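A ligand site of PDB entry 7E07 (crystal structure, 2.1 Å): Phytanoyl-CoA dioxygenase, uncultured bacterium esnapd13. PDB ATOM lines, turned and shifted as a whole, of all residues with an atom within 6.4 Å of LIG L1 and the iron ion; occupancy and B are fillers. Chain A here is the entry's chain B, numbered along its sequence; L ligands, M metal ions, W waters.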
ATOM      1  N   GLN A  99       1.438 -25.191  16.616  1.00  0.00           N
ATOM      2  CA  GLN A  99       0.650 -25.482  15.418  1.00  0.00           C
ATOM      3  C   GLN A  99       1.158 -26.748  14.769  1.00  0.00           C
ATOM      4  O   GLN A  99       2.342 -27.052  14.851  1.00  0.00           O
ATOM      5  CB  GLN A  99       0.743 -24.230  14.487  1.00  0.00           C
ATOM      6  CG  GLN A  99       0.076 -24.369  13.129  1.00  0.00           C
ATOM      7  CD  GLN A  99       0.119 -23.062  12.355  1.00  0.00           C
ATOM      8  OE1 GLN A  99       1.049 -22.813  11.587  1.00  0.00           O
ATOM      9  NE2 GLN A  99      -0.863 -22.188  12.624  1.00  0.00           N
ATOM     10  N   LYS A 101       0.465 -28.777  10.992  1.00  0.00           N
ATOM     11  CA  LYS A 101      -0.232 -28.928   9.722  1.00  0.00           C
ATOM     12  C   LYS A 101       0.429 -29.914   8.773  1.00  0.00           C
ATOM     13  O   LYS A 101       1.629 -30.186   8.876  1.00  0.00           O
ATOM     14  CB  LYS A 101      -0.479 -27.569   9.099  1.00  0.00           C
ATOM     15  CG  LYS A 101       0.749 -26.746   8.927  1.00  0.00           C
ATOM     16  CD  LYS A 101       0.474 -25.250   8.810  1.00  0.00           C
ATOM     17  CE  LYS A 101       1.785 -24.496   8.537  1.00  0.00           C
ATOM     18  NZ  LYS A 101       2.762 -24.319   9.675  1.00  0.00           N
ATOM     19  N   ASN A 103       0.676 -30.164   4.851  1.00  0.00           N
ATOM     20  CA  ASN A 103       0.497 -29.492   3.520  1.00  0.00           C
ATOM     21  C   ASN A 103       0.726 -30.496   2.395  1.00  0.00           C
ATOM     22  O   ASN A 103       1.852 -30.979   2.213  1.00  0.00           O
ATOM     23  CB  ASN A 103       1.434 -28.291   3.367  1.00  0.00           C
ATOM     24  CG  ASN A 103       0.950 -27.063   4.155  1.00  0.00           C
ATOM     25  OD1 ASN A 103      -0.151 -27.028   4.731  1.00  0.00           O
ATOM     26  ND2 ASN A 103       1.768 -26.049   4.157  1.00  0.00           N
ATOM     27  N   LYS A 105       0.425 -30.396  -0.989  1.00  0.00           N
ATOM     28  CA  LYS A 105       1.059 -29.957  -2.234  1.00  0.00           C
ATOM     29  C   LYS A 105       1.027 -31.062  -3.302  1.00  0.00           C
ATOM     30  O   LYS A 105       2.024 -31.689  -3.625  1.00  0.00           O
ATOM     31  CB  LYS A 105       2.463 -29.465  -1.960  1.00  0.00           C
ATOM     32  CG  LYS A 105       3.136 -28.937  -3.198  1.00  0.00           C
ATOM     33  CD  LYS A 105       3.896 -27.685  -2.939  1.00  0.00           C
ATOM     34  CE  LYS A 105       3.052 -26.471  -3.137  1.00  0.00           C
ATOM     35  NZ  LYS A 105       3.976 -25.313  -3.167  1.00  0.00           N
ATOM     36  N   TRP A 113       2.779 -21.321  -2.246  1.00  0.00           N
ATOM     37  CA  TRP A 113       2.834 -20.606  -0.972  1.00  0.00           C
ATOM     38  C   TRP A 113       3.686 -19.376  -1.202  1.00  0.00           C
ATOM     39  O   TRP A 113       4.903 -19.479  -1.465  1.00  0.00           O
ATOM     40  CB  TRP A 113       3.420 -21.523   0.138  1.00  0.00           C
ATOM     41  CG  TRP A 113       2.448 -22.566   0.592  1.00  0.00           C
ATOM     42  CD1 TRP A 113       2.339 -23.871   0.174  1.00  0.00           C
ATOM     43  CD2 TRP A 113       1.439 -22.382   1.573  1.00  0.00           C
ATOM     44  NE1 TRP A 113       1.302 -24.506   0.870  1.00  0.00           N
ATOM     45  CE2 TRP A 113       0.748 -23.587   1.724  1.00  0.00           C
ATOM     46  CE3 TRP A 113       1.061 -21.294   2.358  1.00  0.00           C
ATOM     47  CZ2 TRP A 113      -0.320 -23.716   2.578  1.00  0.00           C
ATOM     48  CZ3 TRP A 113       0.038 -21.447   3.212  1.00  0.00           C
ATOM     49  CH2 TRP A 113      -0.639 -22.632   3.318  1.00  0.00           C
ATOM     50  N   HIS A 116       6.670 -15.585   2.966  1.00  0.00           N
ATOM     51  CA  HIS A 116       6.320 -15.078   4.294  1.00  0.00           C
ATOM     52  C   HIS A 116       7.318 -15.509   5.341  1.00  0.00           C
ATOM     53  O   HIS A 116       8.172 -16.360   5.080  1.00  0.00           O
ATOM     54  CB  HIS A 116       4.948 -15.518   4.664  1.00  0.00           C
ATOM     55  CG  HIS A 116       4.810 -16.993   4.746  1.00  0.00           C
ATOM     56  ND1 HIS A 116       5.022 -17.810   3.670  1.00  0.00           N
ATOM     57  CD2 HIS A 116       4.570 -17.803   5.802  1.00  0.00           C
ATOM     58  CE1 HIS A 116       4.848 -19.072   4.033  1.00  0.00           C
ATOM     59  NE2 HIS A 116       4.589 -19.092   5.327  1.00  0.00           N
ATOM     60  N   GLN A 117       7.224 -14.860   6.496  1.00  0.00           N
ATOM     61  CA  GLN A 117       7.829 -15.353   7.738  1.00  0.00           C
ATOM     62  C   GLN A 117       6.703 -15.842   8.620  1.00  0.00           C
ATOM     63  O   GLN A 117       5.670 -15.146   8.752  1.00  0.00           O
ATOM     64  CB  GLN A 117       8.548 -14.239   8.444  1.00  0.00           C
ATOM     65  CG  GLN A 117       9.731 -13.688   7.664  1.00  0.00           C
ATOM     66  CD  GLN A 117      10.143 -12.323   8.210  1.00  0.00           C
ATOM     67  OE1 GLN A 117      11.304 -12.136   8.661  1.00  0.00           O
ATOM     68  NE2 GLN A 117       9.198 -11.358   8.175  1.00  0.00           N
ATOM     69  N   ASP A 118       6.883 -17.030   9.243  1.00  0.00           N
ATOM     70  CA  ASP A 118       5.801 -17.603  10.087  1.00  0.00           C
ATOM     71  C   ASP A 118       5.501 -16.733  11.336  1.00  0.00           C
ATOM     72  O   ASP A 118       4.343 -16.537  11.741  1.00  0.00           O
ATOM     73  CB  ASP A 118       6.183 -19.025  10.520  1.00  0.00           C
ATOM     74  CG  ASP A 118       6.067 -20.093   9.382  1.00  0.00           C
ATOM     75  OD1 ASP A 118       5.306 -19.868   8.409  1.00  0.00           O
ATOM     76  OD2 ASP A 118       6.743 -21.173   9.478  1.00  0.00           O
ATOM     77  N   TRP A 122       2.146 -15.565  13.634  1.00  0.00           N
ATOM     78  CA  TRP A 122       1.941 -16.074  15.003  1.00  0.00           C
ATOM     79  C   TRP A 122       1.952 -14.877  15.979  1.00  0.00           C
ATOM     80  O   TRP A 122       1.173 -14.830  16.917  1.00  0.00           O
ATOM     81  CB  TRP A 122       2.975 -17.150  15.381  1.00  0.00           C
ATOM     82  CG  TRP A 122       2.954 -18.372  14.458  1.00  0.00           C
ATOM     83  CD1 TRP A 122       1.881 -18.911  13.835  1.00  0.00           C
ATOM     84  CD2 TRP A 122       4.069 -19.140  14.081  1.00  0.00           C
ATOM     85  NE1 TRP A 122       2.258 -20.005  13.074  1.00  0.00           N
ATOM     86  CE2 TRP A 122       3.616 -20.167  13.219  1.00  0.00           C
ATOM     87  CE3 TRP A 122       5.424 -19.125  14.445  1.00  0.00           C
ATOM     88  CZ2 TRP A 122       4.467 -21.146  12.729  1.00  0.00           C
ATOM     89  CZ3 TRP A 122       6.258 -20.094  13.915  1.00  0.00           C
ATOM     90  CH2 TRP A 122       5.791 -21.065  13.053  1.00  0.00           C
ATOM     91  N   GLY A 148       7.858 -28.530  -6.133  1.00  0.00           N
ATOM     92  CA  GLY A 148       7.550 -27.356  -5.346  1.00  0.00           C
ATOM     93  C   GLY A 148       8.173 -27.376  -3.969  1.00  0.00           C
ATOM     94  O   GLY A 148       7.452 -27.255  -2.977  1.00  0.00           O
ATOM     95  N   PRO A 149       9.489 -27.519  -3.901  1.00  0.00           N
ATOM     96  CA  PRO A 149      10.095 -27.626  -2.639  1.00  0.00           C
ATOM     97  C   PRO A 149       9.997 -26.338  -1.844  1.00  0.00           C
ATOM     98  O   PRO A 149       9.987 -25.193  -2.399  1.00  0.00           O
ATOM     99  CB  PRO A 149      11.540 -27.917  -2.962  1.00  0.00           C
ATOM    100  CG  PRO A 149      11.763 -27.252  -4.255  1.00  0.00           C
ATOM    101  CD  PRO A 149      10.496 -27.489  -4.987  1.00  0.00           C
ATOM    102  N   LEU A 150       9.962 -26.542  -0.533  1.00  0.00           N
ATOM    103  CA  LEU A 150      10.007 -25.396   0.382  1.00  0.00           C
ATOM    104  C   LEU A 150      11.317 -24.668   0.157  1.00  0.00           C
ATOM    105  O   LEU A 150      12.426 -25.281   0.208  1.00  0.00           O
ATOM    106  CB  LEU A 150       9.920 -25.895   1.834  1.00  0.00           C
ATOM    107  CG  LEU A 150       9.636 -24.891   2.927  1.00  0.00           C
ATOM    108  CD1 LEU A 150       8.489 -23.989   2.556  1.00  0.00           C
ATOM    109  CD2 LEU A 150       9.250 -25.688   4.189  1.00  0.00           C
ATOM    110  N   THR A 151      11.207 -23.353  -0.042  1.00  0.00           N
ATOM    111  CA  THR A 151      12.376 -22.517  -0.360  1.00  0.00           C
ATOM    112  C   THR A 151      12.629 -21.344   0.541  1.00  0.00           C
ATOM    113  O   THR A 151      11.709 -20.603   0.861  1.00  0.00           O
ATOM    114  CB  THR A 151      12.210 -21.980  -1.819  1.00  0.00           C
ATOM    115  OG1 THR A 151      11.894 -23.076  -2.650  1.00  0.00           O
ATOM    116  CG2 THR A 151      13.486 -21.395  -2.327  1.00  0.00           C
ATOM    117  N   THR A 174      -5.238 -16.859   6.174  1.00  0.00           N
ATOM    118  CA  THR A 174      -3.890 -17.202   6.729  1.00  0.00           C
ATOM    119  C   THR A 174      -3.345 -18.552   6.158  1.00  0.00           C
ATOM    120  O   THR A 174      -2.135 -18.842   6.198  1.00  0.00           O
ATOM    121  CB  THR A 174      -3.916 -17.239   8.286  1.00  0.00           C
ATOM    122  OG1 THR A 174      -4.940 -18.150   8.770  1.00  0.00           O
ATOM    123  CG2 THR A 174      -4.111 -15.824   8.884  1.00  0.00           C
ATOM    124  N   PHE A 210      13.286 -25.515  10.569  1.00  0.00           N
ATOM    125  CA  PHE A 210      13.484 -24.093  10.242  1.00  0.00           C
ATOM    126  C   PHE A 210      12.906 -23.083  11.218  1.00  0.00           C
ATOM    127  O   PHE A 210      11.844 -23.262  11.853  1.00  0.00           O
ATOM    128  CB  PHE A 210      13.003 -23.750   8.794  1.00  0.00           C
ATOM    129  CG  PHE A 210      11.522 -23.958   8.513  1.00  0.00           C
ATOM    130  CD1 PHE A 210      11.058 -25.153   8.143  1.00  0.00           C
ATOM    131  CD2 PHE A 210      10.617 -22.919   8.569  1.00  0.00           C
ATOM    132  CE1 PHE A 210       9.729 -25.360   7.865  1.00  0.00           C
ATOM    133  CE2 PHE A 210       9.296 -23.108   8.232  1.00  0.00           C
ATOM    134  CZ  PHE A 210       8.846 -24.342   7.892  1.00  0.00           C
ATOM    135  N   HIS A 216      10.430 -17.865   3.546  1.00  0.00           N
ATOM    136  CA  HIS A 216      10.325 -19.063   2.797  1.00  0.00           C
ATOM    137  C   HIS A 216       9.089 -18.977   1.958  1.00  0.00           C
ATOM    138  O   HIS A 216       8.248 -18.148   2.194  1.00  0.00           O
ATOM    139  CB  HIS A 216      10.240 -20.315   3.725  1.00  0.00           C
ATOM    140  CG  HIS A 216       9.098 -20.314   4.715  1.00  0.00           C
ATOM    141  ND1 HIS A 216       9.162 -19.639   5.921  1.00  0.00           N
ATOM    142  CD2 HIS A 216       7.913 -20.987   4.718  1.00  0.00           C
ATOM    143  CE1 HIS A 216       8.026 -19.837   6.587  1.00  0.00           C
ATOM    144  NE2 HIS A 216       7.259 -20.663   5.892  1.00  0.00           N
ATOM    145  N   SER A 217       8.987 -19.915   1.045  1.00  0.00           N
ATOM    146  CA  SER A 217       8.073 -19.915  -0.089  1.00  0.00           C
ATOM    147  C   SER A 217       8.051 -21.271  -0.763  1.00  0.00           C
ATOM    148  O   SER A 217       8.995 -22.049  -0.587  1.00  0.00           O
ATOM    149  CB  SER A 217       8.592 -18.960  -1.199  1.00  0.00           C
ATOM    150  OG  SER A 217       7.380 -18.697  -1.889  1.00  0.00           O
ATOM    151  N   SER A 218       7.038 -21.539  -1.596  1.00  0.00           N
ATOM    152  CA  SER A 218       7.117 -22.665  -2.492  1.00  0.00           C
ATOM    153  C   SER A 218       6.276 -22.440  -3.783  1.00  0.00           C
ATOM    154  O   SER A 218       5.170 -21.900  -3.759  1.00  0.00           O
ATOM    155  CB  SER A 218       6.693 -23.934  -1.752  1.00  0.00           C
ATOM    156  OG  SER A 218       5.293 -23.808  -1.399  1.00  0.00           O
ATOM    157  N   VAL A 219       6.805 -22.893  -4.888  1.00  0.00           N
ATOM    158  CA  VAL A 219       6.141 -22.659  -6.195  1.00  0.00           C
ATOM    159  C   VAL A 219       5.102 -23.745  -6.417  1.00  0.00           C
ATOM    160  O   VAL A 219       5.139 -24.757  -5.712  1.00  0.00           O
ATOM    161  CB  VAL A 219       7.151 -22.607  -7.376  1.00  0.00           C
ATOM    162  CG1 VAL A 219       8.261 -21.635  -7.047  1.00  0.00           C
ATOM    163  CG2 VAL A 219       7.708 -23.997  -7.704  1.00  0.00           C
ATOM    164  N   ARG A 227       4.072 -33.821  -2.856  1.00  0.00           N
ATOM    165  CA  ARG A 227       5.105 -33.347  -1.961  1.00  0.00           C
ATOM    166  C   ARG A 227       4.459 -33.078  -0.556  1.00  0.00           C
ATOM    167  O   ARG A 227       4.402 -31.962  -0.048  1.00  0.00           O
ATOM    168  CB  ARG A 227       5.836 -32.187  -2.654  1.00  0.00           C
ATOM    169  CG  ARG A 227       7.067 -31.585  -1.946  1.00  0.00           C
ATOM    170  CD  ARG A 227       6.517 -30.696  -0.893  1.00  0.00           C
ATOM    171  NE  ARG A 227       6.677 -29.286  -0.931  1.00  0.00           N
ATOM    172  CZ  ARG A 227       5.918 -28.439  -0.204  1.00  0.00           C
ATOM    173  NH1 ARG A 227       4.858 -28.811   0.511  1.00  0.00           N
ATOM    174  NH2 ARG A 227       6.191 -27.178  -0.285  1.00  0.00           N
ATOM    175  N   LEU A 229       4.121 -32.676   3.218  1.00  0.00           N
ATOM    176  CA  LEU A 229       4.957 -32.294   4.419  1.00  0.00           C
ATOM    177  C   LEU A 229       4.086 -32.344   5.653  1.00  0.00           C
ATOM    178  O   LEU A 229       2.966 -31.803   5.614  1.00  0.00           O
ATOM    179  CB  LEU A 229       5.510 -30.868   4.259  1.00  0.00           C
ATOM    180  CG  LEU A 229       6.440 -30.726   3.054  1.00  0.00           C
ATOM    181  CD1 LEU A 229       6.933 -29.305   3.017  1.00  0.00           C
ATOM    182  CD2 LEU A 229       7.646 -31.601   3.194  1.00  0.00           C
ATOM    183  N   LEU A 231       4.130 -30.631   9.056  1.00  0.00           N
ATOM    184  CA  LEU A 231       4.882 -29.510   9.711  1.00  0.00           C
ATOM    185  C   LEU A 231       4.479 -29.386  11.159  1.00  0.00           C
ATOM    186  O   LEU A 231       3.288 -29.148  11.490  1.00  0.00           O
ATOM    187  CB  LEU A 231       4.671 -28.158   9.037  1.00  0.00           C
ATOM    188  CG  LEU A 231       5.150 -28.149   7.561  1.00  0.00           C
ATOM    189  CD1 LEU A 231       3.942 -28.141   6.668  1.00  0.00           C
ATOM    190  CD2 LEU A 231       6.009 -26.965   7.257  1.00  0.00           C
HETATM  191  C1  LIG L   1       3.334 -22.671   5.981  1.00  0.00           C
HETATM  192  O1  LIG L   1       2.227 -23.341   5.910  1.00  0.00           O
HETATM  193  O2  LIG L   1       3.630 -21.683   6.710  1.00  0.00           O
HETATM  194  C2  LIG L   1       4.389 -22.997   5.035  1.00  0.00           C
HETATM  195  O3  LIG L   1       5.416 -22.334   5.010  1.00  0.00           O
HETATM  196  C3  LIG L   1       4.083 -24.102   4.064  1.00  0.00           C
HETATM  197  C4  LIG L   1       4.887 -23.987   2.834  1.00  0.00           C
HETATM  198  C5  LIG L   1       4.861 -25.215   1.951  1.00  0.00           C
HETATM  199  O4  LIG L   1       4.185 -26.236   2.176  1.00  0.00           O
HETATM  200  O5  LIG L   1       5.634 -25.123   0.971  1.00  0.00           O
HETATM  201  N1  LG2 L   2      -0.086 -20.253   7.660  1.00  0.00           N
HETATM  202  C1  LG2 L   2       0.282 -20.545   9.078  1.00  0.00           C
HETATM  203  C2  LG2 L   2      -0.469 -19.674  10.050  1.00  0.00           C
HETATM  204  O1  LG2 L   2      -1.432 -18.991   9.640  1.00  0.00           O
HETATM  205  C3  LG2 L   2       1.752 -20.138   9.145  1.00  0.00           C
HETATM  206  C4  LG2 L   2       1.882 -19.044   8.139  1.00  0.00           C
HETATM  207  C5  LG2 L   2       0.896 -19.363   7.035  1.00  0.00           C
HETATM  208  O2  LG2 L   2      -0.058 -19.587  11.207  1.00  0.00           O
HETATM  209 FE    FE M   1       5.292 -20.905   6.598  1.00  0.00          FE
HETATM  210  O   HOH W   1      -0.355 -22.989   6.720  1.00  0.00           O
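The nearest printed residue that does not touch the iron ion is Phe 210 (4.9 Å).
NH2 of Arg 227 is in salt-bridge range of O5 of LIG L1. O5 of LIG L1 lies within hydrogen-bond range of OG of Ser 218 (2.7 Å). NZ of Lys 101 lies within salt-bridge range of O1 of LIG L1, 3.9 Å away. ND2 of Asn 103 lies close to O4 of LIG L1, at 3.1 Å. An oxygen (O2) of LG2 L2 sits at hydrogen-bond distance from the side-chain amide nitrogen (NE2) of Gln 99, at 3.1 Å. The indole nitrogen (NE1) of Trp 122 is in hydrogen-bond range of an oxygen (O2) of LG2 L2 (3.0 Å). A nitrogen (N1) of LG2 L2 sits at hydrogen-bond distance from the backbone carbonyl oxygen (O) of Thr 174, 2.9 Å away.
The iron ion is bound by an oxygen (O2) of LIG L1 (1.8 Å), the side-chain carboxylate (OD1) of Asp 118 (2.1 Å), a ring nitrogen (NE2) of His 216 (2.1 Å), an oxygen (O3) of LIG L1 (2.1 Å) and a ring nitrogen (NE2) of His 116 (2.3 Å). The iron ion has five donor atoms within binding distance.
Residues that only touch LIG L1: Trp 113 and Leu 150. Nine residues have an atom within 4 Å of LIG L1: Lys 101, Asn 103, Trp 113, His 116, Asp 118, Leu 150, His 216, Ser 218 and Arg 227.
N of Arg 227 sits at hydrogen-bond distance from O of Lys 105, at 3.1 Å. The guanidinium group of Arg 227 is in hydrogen-bond range of the backbone carbonyl oxygen of Gly 148 (3.0 Å). O of Ser 218 lies within hydrogen-bond range of N of Trp 113 (2.9 Å). The side-chain amino group of Lys 105 is in hydrogen-bond range of the side-chain hydroxyl of Ser 218. N of Leu 231 is in hydrogen-bond range of O of Lys 101. OE1 of Gln 99 is in hydrogen-bond range of NZ of Lys 101 (3.0 Å). The backbone NH (N) of Asn 103 is in hydrogen-bond range of the backbone carbonyl oxygen (O) of Leu 229, at 2.9 Å. The backbone carbonyl oxygen of Trp 113 is in hydrogen-bond range of the side-chain hydroxyl of Ser 217 (2.6 Å).
Water W1 lies within hydrogen-bond range of O1 of LIG L1 and N1 of LG2 L2.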
